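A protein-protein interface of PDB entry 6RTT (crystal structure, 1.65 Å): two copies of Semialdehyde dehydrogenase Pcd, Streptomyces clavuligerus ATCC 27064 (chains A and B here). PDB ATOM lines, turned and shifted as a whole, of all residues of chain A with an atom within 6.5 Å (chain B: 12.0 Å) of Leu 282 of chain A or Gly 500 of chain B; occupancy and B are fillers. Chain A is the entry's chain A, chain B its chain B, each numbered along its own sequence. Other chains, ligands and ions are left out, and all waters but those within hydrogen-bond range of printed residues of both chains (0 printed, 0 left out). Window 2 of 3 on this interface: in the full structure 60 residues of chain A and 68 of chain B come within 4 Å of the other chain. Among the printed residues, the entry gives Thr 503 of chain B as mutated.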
ATOM      1  N   ASP A 279       2.872   0.919 -15.969  1.00  0.00           N
ATOM      2  CA  ASP A 279       1.618   0.249 -16.303  1.00  0.00           C
ATOM      3  C   ASP A 279       0.964  -0.194 -15.000  1.00  0.00           C
ATOM      4  O   ASP A 279       1.452  -1.117 -14.336  1.00  0.00           O
ATOM      5  CB  ASP A 279       1.923  -0.925 -17.231  1.00  0.00           C
ATOM      6  CG  ASP A 279       0.697  -1.763 -17.598  1.00  0.00           C
ATOM      7  OD1 ASP A 279      -0.244  -1.901 -16.799  1.00  0.00           O
ATOM      8  OD2 ASP A 279       0.697  -2.312 -18.721  1.00  0.00           O
ATOM      9  N   LEU A 280      -0.136   0.465 -14.618  1.00  0.00           N
ATOM     10  CA  LEU A 280      -0.659   0.273 -13.266  1.00  0.00           C
ATOM     11  C   LEU A 280      -1.319  -1.089 -13.081  1.00  0.00           C
ATOM     12  O   LEU A 280      -1.261  -1.651 -11.983  1.00  0.00           O
ATOM     13  CB  LEU A 280      -1.629   1.395 -12.897  1.00  0.00           C
ATOM     14  CG  LEU A 280      -0.973   2.767 -12.694  1.00  0.00           C
ATOM     15  CD1 LEU A 280      -1.965   3.776 -12.127  1.00  0.00           C
ATOM     16  CD2 LEU A 280       0.267   2.678 -11.814  1.00  0.00           C
ATOM     17  N   ASP A 281      -1.946  -1.642 -14.123  1.00  0.00           N
ATOM     18  CA  ASP A 281      -2.473  -2.999 -14.011  1.00  0.00           C
ATOM     19  C   ASP A 281      -1.344  -4.005 -13.795  1.00  0.00           C
ATOM     20  O   ASP A 281      -1.428  -4.870 -12.915  1.00  0.00           O
ATOM     21  CB  ASP A 281      -3.285  -3.357 -15.255  1.00  0.00           C
ATOM     22  CG  ASP A 281      -4.674  -2.728 -15.256  1.00  0.00           C
ATOM     23  OD1 ASP A 281      -4.963  -1.873 -14.391  1.00  0.00           O
ATOM     24  OD2 ASP A 281      -5.479  -3.096 -16.137  1.00  0.00           O
ATOM     25  N   LEU A 282      -0.283  -3.911 -14.600  1.00  0.00           N
ATOM     26  CA  LEU A 282       0.893  -4.748 -14.379  1.00  0.00           C
ATOM     27  C   LEU A 282       1.445  -4.542 -12.973  1.00  0.00           C
ATOM     28  O   LEU A 282       1.693  -5.508 -12.241  1.00  0.00           O
ATOM     29  CB  LEU A 282       1.967  -4.444 -15.430  1.00  0.00           C
ATOM     30  CG  LEU A 282       3.384  -4.961 -15.137  1.00  0.00           C
ATOM     31  CD1 LEU A 282       3.411  -6.468 -15.213  1.00  0.00           C
ATOM     32  CD2 LEU A 282       4.431  -4.346 -16.078  1.00  0.00           C
ATOM     33  N   THR A 283       1.613  -3.278 -12.570  1.00  0.00           N
ATOM     34  CA  THR A 283       2.284  -2.976 -11.305  1.00  0.00           C
ATOM     35  C   THR A 283       1.478  -3.461 -10.105  1.00  0.00           C
ATOM     36  O   THR A 283       2.043  -4.020  -9.156  1.00  0.00           O
ATOM     37  CB  THR A 283       2.549  -1.473 -11.201  1.00  0.00           C
ATOM     38  OG1 THR A 283       3.363  -1.058 -12.306  1.00  0.00           O
ATOM     39  CG2 THR A 283       3.276  -1.140  -9.899  1.00  0.00           C
ATOM     40  N   VAL A 284       0.158  -3.250 -10.116  1.00  0.00           N
ATOM     41  CA  VAL A 284      -0.646  -3.673  -8.973  1.00  0.00           C
ATOM     42  C   VAL A 284      -0.633  -5.191  -8.839  1.00  0.00           C
ATOM     43  O   VAL A 284      -0.468  -5.721  -7.734  1.00  0.00           O
ATOM     44  CB  VAL A 284      -2.078  -3.118  -9.081  1.00  0.00           C
ATOM     45  CG1 VAL A 284      -2.965  -3.765  -8.021  1.00  0.00           C
ATOM     46  CG2 VAL A 284      -2.057  -1.607  -8.904  1.00  0.00           C
ATOM     47  N   ASN A 285      -0.785  -5.913  -9.954  1.00  0.00           N
ATOM     48  CA  ASN A 285      -0.721  -7.373  -9.908  1.00  0.00           C
ATOM     49  C   ASN A 285       0.636  -7.852  -9.403  1.00  0.00           C
ATOM     50  O   ASN A 285       0.714  -8.733  -8.535  1.00  0.00           O
ATOM     51  CB  ASN A 285      -1.007  -7.965 -11.291  1.00  0.00           C
ATOM     52  CG  ASN A 285      -2.489  -7.983 -11.627  1.00  0.00           C
ATOM     53  OD1 ASN A 285      -3.343  -8.009 -10.741  1.00  0.00           O
ATOM     54  ND2 ASN A 285      -2.799  -7.974 -12.918  1.00  0.00           N
ATOM     55  N   ALA A 286       1.721  -7.293  -9.946  1.00  0.00           N
ATOM     56  CA  ALA A 286       3.053  -7.724  -9.536  1.00  0.00           C
ATOM     57  C   ALA A 286       3.299  -7.423  -8.065  1.00  0.00           C
ATOM     58  O   ALA A 286       3.894  -8.235  -7.345  1.00  0.00           O
ATOM     59  CB  ALA A 286       4.117  -7.040 -10.400  1.00  0.00           C
ATOM     60  N   ALA A 287       2.853  -6.253  -7.604  1.00  0.00           N
ATOM     61  CA  ALA A 287       3.096  -5.864  -6.222  1.00  0.00           C
ATOM     62  C   ALA A 287       2.306  -6.735  -5.254  1.00  0.00           C
ATOM     63  O   ALA A 287       2.830  -7.134  -4.210  1.00  0.00           O
ATOM     64  CB  ALA A 287       2.753  -4.394  -6.017  1.00  0.00           C
ATOM     65  N   PHE A 432       9.163  -0.283 -11.965  1.00  0.00           N
ATOM     66  CA  PHE A 432       8.074  -0.368 -12.927  1.00  0.00           C
ATOM     67  C   PHE A 432       8.004   0.955 -13.659  1.00  0.00           C
ATOM     68  O   PHE A 432       7.781   2.000 -13.041  1.00  0.00           O
ATOM     69  CB  PHE A 432       6.766  -0.715 -12.223  1.00  0.00           C
ATOM     70  CG  PHE A 432       6.764  -2.102 -11.683  1.00  0.00           C
ATOM     71  CD1 PHE A 432       7.341  -2.377 -10.446  1.00  0.00           C
ATOM     72  CD2 PHE A 432       6.260  -3.150 -12.428  1.00  0.00           C
ATOM     73  CE1 PHE A 432       7.383  -3.676  -9.955  1.00  0.00           C
ATOM     74  CE2 PHE A 432       6.298  -4.454 -11.938  1.00  0.00           C
ATOM     75  CZ  PHE A 432       6.859  -4.712 -10.707  1.00  0.00           C
ATOM     76  N   ASN A 456      10.202  -3.979 -14.504  1.00  0.00           N
ATOM     77  CA  ASN A 456       8.827  -4.400 -14.805  1.00  0.00           C
ATOM     78  C   ASN A 456       8.531  -5.836 -14.389  1.00  0.00           C
ATOM     79  O   ASN A 456       7.624  -6.477 -14.940  1.00  0.00           O
ATOM     80  CB  ASN A 456       8.501  -4.171 -16.284  1.00  0.00           C
ATOM     81  CG  ASN A 456       8.329  -2.706 -16.576  1.00  0.00           C
ATOM     82  OD1 ASN A 456       7.872  -1.971 -15.702  1.00  0.00           O
ATOM     83  ND2 ASN A 456       8.732  -2.255 -17.767  1.00  0.00           N
ATOM     84  N   ILE A 457       9.282  -6.335 -13.411  1.00  0.00           N
ATOM     85  CA  ILE A 457       8.973  -7.574 -12.714  1.00  0.00           C
ATOM     86  C   ILE A 457       9.396  -7.359 -11.267  1.00  0.00           C
ATOM     87  O   ILE A 457      10.316  -6.586 -10.980  1.00  0.00           O
ATOM     88  CB  ILE A 457       9.653  -8.803 -13.388  1.00  0.00           C
ATOM     89  CG1 ILE A 457       9.366 -10.095 -12.624  1.00  0.00           C
ATOM     90  CG2 ILE A 457      11.153  -8.589 -13.568  1.00  0.00           C
ATOM     91  CD1 ILE A 457       9.775 -11.357 -13.392  1.00  0.00           C
ATOM     92  N   ARG B 142      11.319 -16.916 -18.958  1.00  0.00           N
ATOM     93  CA  ARG B 142      10.098 -16.123 -19.059  1.00  0.00           C
ATOM     94  C   ARG B 142       9.942 -15.565 -20.471  1.00  0.00           C
ATOM     95  O   ARG B 142      10.842 -14.860 -20.949  1.00  0.00           O
ATOM     96  CB  ARG B 142      10.128 -14.978 -18.051  1.00  0.00           C
ATOM     97  CG  ARG B 142      10.494 -15.408 -16.632  1.00  0.00           C
ATOM     98  CD  ARG B 142      10.658 -14.200 -15.729  1.00  0.00           C
ATOM     99  NE  ARG B 142      11.180 -14.586 -14.419  1.00  0.00           N
ATOM    100  CZ  ARG B 142      10.422 -15.002 -13.407  1.00  0.00           C
ATOM    101  NH1 ARG B 142       9.102 -15.085 -13.544  1.00  0.00           N
ATOM    102  NH2 ARG B 142      10.986 -15.339 -12.254  1.00  0.00           N
ATOM    103  N   PRO B 143       8.835 -15.837 -21.162  1.00  0.00           N
ATOM    104  CA  PRO B 143       8.622 -15.229 -22.483  1.00  0.00           C
ATOM    105  C   PRO B 143       8.629 -13.708 -22.403  1.00  0.00           C
ATOM    106  O   PRO B 143       8.081 -13.116 -21.475  1.00  0.00           O
ATOM    107  CB  PRO B 143       7.239 -15.753 -22.893  1.00  0.00           C
ATOM    108  CG  PRO B 143       7.062 -17.022 -22.104  1.00  0.00           C
ATOM    109  CD  PRO B 143       7.771 -16.792 -20.799  1.00  0.00           C
ATOM    110  N   GLY B 144       9.256 -13.073 -23.387  1.00  0.00           N
ATOM    111  CA  GLY B 144       9.202 -11.621 -23.441  1.00  0.00           C
ATOM    112  C   GLY B 144       9.992 -10.923 -22.357  1.00  0.00           C
ATOM    113  O   GLY B 144       9.710  -9.765 -22.034  1.00  0.00           O
ATOM    114  N   HIS B 145      10.963 -11.609 -21.766  1.00  0.00           N
ATOM    115  CA  HIS B 145      11.898 -11.053 -20.801  1.00  0.00           C
ATOM    116  C   HIS B 145      13.317 -11.261 -21.316  1.00  0.00           C
ATOM    117  O   HIS B 145      13.559 -12.054 -22.233  1.00  0.00           O
ATOM    118  CB  HIS B 145      11.779 -11.727 -19.426  1.00  0.00           C
ATOM    119  CG  HIS B 145      10.470 -11.512 -18.721  1.00  0.00           C
ATOM    120  ND1 HIS B 145       9.251 -11.840 -19.278  1.00  0.00           N
ATOM    121  CD2 HIS B 145      10.204 -11.070 -17.470  1.00  0.00           C
ATOM    122  CE1 HIS B 145       8.290 -11.593 -18.404  1.00  0.00           C
ATOM    123  NE2 HIS B 145       8.842 -11.126 -17.298  1.00  0.00           N
ATOM    124  N   ARG B 146      14.257 -10.548 -20.697  1.00  0.00           N
ATOM    125  CA  ARG B 146      15.687 -10.683 -20.949  1.00  0.00           C
ATOM    126  C   ARG B 146      16.401 -10.785 -19.602  1.00  0.00           C
ATOM    127  O   ARG B 146      15.929 -10.246 -18.598  1.00  0.00           O
ATOM    128  CB  ARG B 146      16.217  -9.475 -21.766  1.00  0.00           C
ATOM    129  CG  ARG B 146      17.653  -9.593 -22.230  1.00  0.00           C
ATOM    130  CD  ARG B 146      18.084  -8.409 -23.096  1.00  0.00           C
ATOM    131  NE  ARG B 146      17.928  -7.112 -22.433  1.00  0.00           N
ATOM    132  CZ  ARG B 146      18.779  -6.643 -21.528  1.00  0.00           C
ATOM    133  NH1 ARG B 146      19.826  -7.378 -21.171  1.00  0.00           N
ATOM    134  NH2 ARG B 146      18.585  -5.453 -20.977  1.00  0.00           N
ATOM    135  N   THR B 495      16.729  -9.095 -14.374  1.00  0.00           N
ATOM    136  CA  THR B 495      15.675  -9.566 -15.276  1.00  0.00           C
ATOM    137  C   THR B 495      14.881  -8.357 -15.758  1.00  0.00           C
ATOM    138  O   THR B 495      14.468  -7.525 -14.945  1.00  0.00           O
ATOM    139  CB  THR B 495      14.740 -10.569 -14.593  1.00  0.00           C
ATOM    140  OG1 THR B 495      15.502 -11.676 -14.079  1.00  0.00           O
ATOM    141  CG2 THR B 495      13.694 -11.103 -15.603  1.00  0.00           C
ATOM    142  N   VAL B 496      14.665  -8.269 -17.073  1.00  0.00           N
ATOM    143  CA  VAL B 496      13.967  -7.146 -17.694  1.00  0.00           C
ATOM    144  C   VAL B 496      12.748  -7.686 -18.425  1.00  0.00           C
ATOM    145  O   VAL B 496      12.876  -8.491 -19.357  1.00  0.00           O
ATOM    146  CB  VAL B 496      14.878  -6.368 -18.660  1.00  0.00           C
ATOM    147  CG1 VAL B 496      14.085  -5.309 -19.402  1.00  0.00           C
ATOM    148  CG2 VAL B 496      16.046  -5.763 -17.900  1.00  0.00           C
ATOM    149  N   ASN B 497      11.571  -7.227 -18.016  1.00  0.00           N
ATOM    150  CA  ASN B 497      10.316  -7.594 -18.669  1.00  0.00           C
ATOM    151  C   ASN B 497       9.989  -6.538 -19.714  1.00  0.00           C
ATOM    152  O   ASN B 497       9.885  -5.354 -19.386  1.00  0.00           O
ATOM    153  CB  ASN B 497       9.205  -7.689 -17.624  1.00  0.00           C
ATOM    154  CG  ASN B 497       7.864  -8.064 -18.215  1.00  0.00           C
ATOM    155  OD1 ASN B 497       7.773  -8.568 -19.338  1.00  0.00           O
ATOM    156  ND2 ASN B 497       6.806  -7.833 -17.445  1.00  0.00           N
ATOM    157  N   TYR B 498       9.829  -6.952 -20.970  1.00  0.00           N
ATOM    158  CA  TYR B 498       9.395  -6.004 -21.987  1.00  0.00           C
ATOM    159  C   TYR B 498       8.082  -6.427 -22.619  1.00  0.00           C
ATOM    160  O   TYR B 498       7.696  -5.863 -23.645  1.00  0.00           O
ATOM    161  CB  TYR B 498      10.477  -5.809 -23.059  1.00  0.00           C
ATOM    162  CG  TYR B 498      10.932  -7.062 -23.781  1.00  0.00           C
ATOM    163  CD1 TYR B 498      10.300  -7.485 -24.943  1.00  0.00           C
ATOM    164  CD2 TYR B 498      12.019  -7.801 -23.316  1.00  0.00           C
ATOM    165  CE1 TYR B 498      10.718  -8.614 -25.612  1.00  0.00           C
ATOM    166  CE2 TYR B 498      12.451  -8.936 -23.985  1.00  0.00           C
ATOM    167  CZ  TYR B 498      11.789  -9.338 -25.129  1.00  0.00           C
ATOM    168  OH  TYR B 498      12.203 -10.462 -25.799  1.00  0.00           O
ATOM    169  N   SER B 499       7.381  -7.387 -22.009  1.00  0.00           N
ATOM    170  CA  SER B 499       6.150  -7.963 -22.534  1.00  0.00           C
ATOM    171  C   SER B 499       4.904  -7.320 -21.953  1.00  0.00           C
ATOM    172  O   SER B 499       3.804  -7.584 -22.449  1.00  0.00           O
ATOM    173  CB  SER B 499       6.102  -9.465 -22.238  1.00  0.00           C
ATOM    174  OG  SER B 499       5.730  -9.688 -20.880  1.00  0.00           O
ATOM    175  N   GLY B 500       5.044  -6.528 -20.895  1.00  0.00           N
ATOM    176  CA  GLY B 500       3.920  -5.854 -20.289  1.00  0.00           C
ATOM    177  C   GLY B 500       3.039  -6.717 -19.420  1.00  0.00           C
ATOM    178  O   GLY B 500       1.981  -6.246 -18.985  1.00  0.00           O
ATOM    179  N   ARG B 501       3.432  -7.957 -19.131  1.00  0.00           N
ATOM    180  CA  ARG B 501       2.559  -8.859 -18.398  1.00  0.00           C
ATOM    181  C   ARG B 501       3.319  -9.537 -17.263  1.00  0.00           C
ATOM    182  O   ARG B 501       4.552  -9.601 -17.255  1.00  0.00           O
ATOM    183  CB  ARG B 501       1.921  -9.901 -19.335  1.00  0.00           C
ATOM    184  CG  ARG B 501       2.897 -10.825 -20.034  1.00  0.00           C
ATOM    185  CD  ARG B 501       2.165 -11.937 -20.786  1.00  0.00           C
ATOM    186  NE  ARG B 501       0.967 -12.421 -20.093  1.00  0.00           N
ATOM    187  CZ  ARG B 501       0.962 -13.110 -18.951  1.00  0.00           C
ATOM    188  NH1 ARG B 501       2.102 -13.406 -18.341  1.00  0.00           N
ATOM    189  NH2 ARG B 501      -0.194 -13.503 -18.430  1.00  0.00           N
ATOM    190  N   VAL B 502       2.544 -10.021 -16.284  1.00  0.00           N
ATOM    191  CA  VAL B 502       3.034 -10.754 -15.122  1.00  0.00           C
ATOM    192  C   VAL B 502       2.146 -11.977 -14.937  1.00  0.00           C
ATOM    193  O   VAL B 502       0.952 -11.952 -15.254  1.00  0.00           O
ATOM    194  CB  VAL B 502       3.049  -9.874 -13.838  1.00  0.00           C
ATOM    195  CG1 VAL B 502       1.700  -9.190 -13.613  1.00  0.00           C
ATOM    196  CG2 VAL B 502       3.452 -10.684 -12.599  1.00  0.00           C
ATOM    197  N   THR B 503       2.739 -13.063 -14.442  1.00  0.00           N
ATOM    198  CA  THR B 503       1.966 -14.260 -14.136  1.00  0.00           C
ATOM    199  C   THR B 503       0.907 -13.964 -13.078  1.00  0.00           C
ATOM    200  O   THR B 503       1.171 -13.287 -12.079  1.00  0.00           O
ATOM    201  CB  THR B 503       2.890 -15.381 -13.655  1.00  0.00           C
ATOM    202  OG1 THR B 503       3.873 -15.653 -14.660  1.00  0.00           O
ATOM    203  CG2 THR B 503       2.097 -16.654 -13.366  1.00  0.00           C
ATOM    204  N   LEU B 504      -0.299 -14.472 -13.309  1.00  0.00           N
ATOM    205  CA  LEU B 504      -1.401 -14.316 -12.369  1.00  0.00           C
ATOM    206  C   LEU B 504      -1.589 -15.577 -11.531  1.00  0.00           C
ATOM    207  O   LEU B 504      -1.935 -16.637 -12.055  1.00  0.00           O
ATOM    208  CB  LEU B 504      -2.692 -13.977 -13.117  1.00  0.00           C
ATOM    209  CG  LEU B 504      -2.589 -12.797 -14.085  1.00  0.00           C
ATOM    210  CD1 LEU B 504      -3.675 -12.871 -15.149  1.00  0.00           C
ATOM    211  CD2 LEU B 504      -2.658 -11.482 -13.323  1.00  0.00           C
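O of Asn 456 of chain A is in hydrogen-bond range of ND2 of Asn 497 of chain B.
The side-chain carboxylate (OD1) of Asp 279 of chain A is in hydrogen-bond range of the backbone NH (N) of Leu 282 of chain A, at 3.0 Å. The side-chain hydroxyl (OG) of Ser 499 of chain B sits close to the backbone NH (N) of Arg 501 of chain B, at 3.4 Å. The backbone carbonyl oxygen of Asp 281 of chain A is in hydrogen-bond range of the side-chain amide nitrogen of Asn 285 of chain A (3.4 Å). The side-chain amide oxygen (OD1) of Asn 497 of chain B sits at hydrogen-bond distance from the side-chain hydroxyl (OG) of Ser 499 of chain B (2.8 Å). OD1 of Asn 497 of chain B lies close to NE2 of His 145 of chain B, 3.4 Å away. ND2 of Asn 497 of chain B is in hydrogen-bond range of O of Arg 501 of chain B (2.9 Å).
Among the printed residues, pairs that only touch across the chains: Leu 282 of chain A with Gly 500 of chain B (3.99 Å), Leu 282 of chain A with Arg 501 of chain B (3.7 Å), Leu 282 of chain A with Val 502 of chain B (3.6 Å), Asn 285 of chain A with Val 502 of chain B (3.8 Å), Asn 285 of chain A with Leu 504 of chain B (3.5 Å), Ile 457 of chain A with Arg 142 of chain B (3.7 Å) and Ile 457 of chain A with Thr 495 of chain B (3.7 Å).
Printed residues of chain B within 4 Å of Leu 282 of chain A: Gly 500 (3.99 Å), Arg 501 (3.7 Å) and Val 502 (3.6 Å). Printed residues of chain A within 4 Å of Gly 500 of chain B: Leu 282. No residue of chain B comes within 4 Å of Thr 283 of chain A. Ala 286 of chain A touches none of the printed residues of chain B. Phe 432 of chain A touches none of the printed residues of chain B. Asn 456 of chain A touches just one residue of chain B: Asn 497 (3.0 Å). Of the printed residues of chain B, Ile 457 of chain A touches Arg 142 and Thr 495. Printed residues of chain A within 4 Å of Arg 501 of chain B: Leu 282. Of the printed residues of chain A, Val 502 of chain B touches Leu 282 (3.6 Å) and Asn 285 (3.8 Å). Of the printed residues of chain A, Arg 142 of chain B touches Ile 457. Printed residues of chain A within 4 Å of Asn 497 of chain B: Asn 456 (3.0 Å). The nearest printed residue of chain B that does not touch Leu 282 of chain A is Asn 497 of chain B (4.3 Å). The nearest printed residue of chain B that does not touch Ile 457 of chain A is His 145 of chain B (4.02 Å).
Printed residues of chain B that touch a printed residue of chain A: Arg 142, Thr 495, Asn 497, Gly 500, Arg 501, Val 502 and Leu 504. Of the 12 printed residues of chain A, 4 touch a printed residue of chain B. Among the printed residues, 8 pairs touch across the chains. Among the printed residues, no Asp or Glu carboxylate lies within 4 Å of a Lys or Arg side-chain nitrogen of the other chain.
No position is printed for both chains. Of the 8 pairs that touch across the chains among the printed residues, none has its exchanged pair printed and touching as well.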
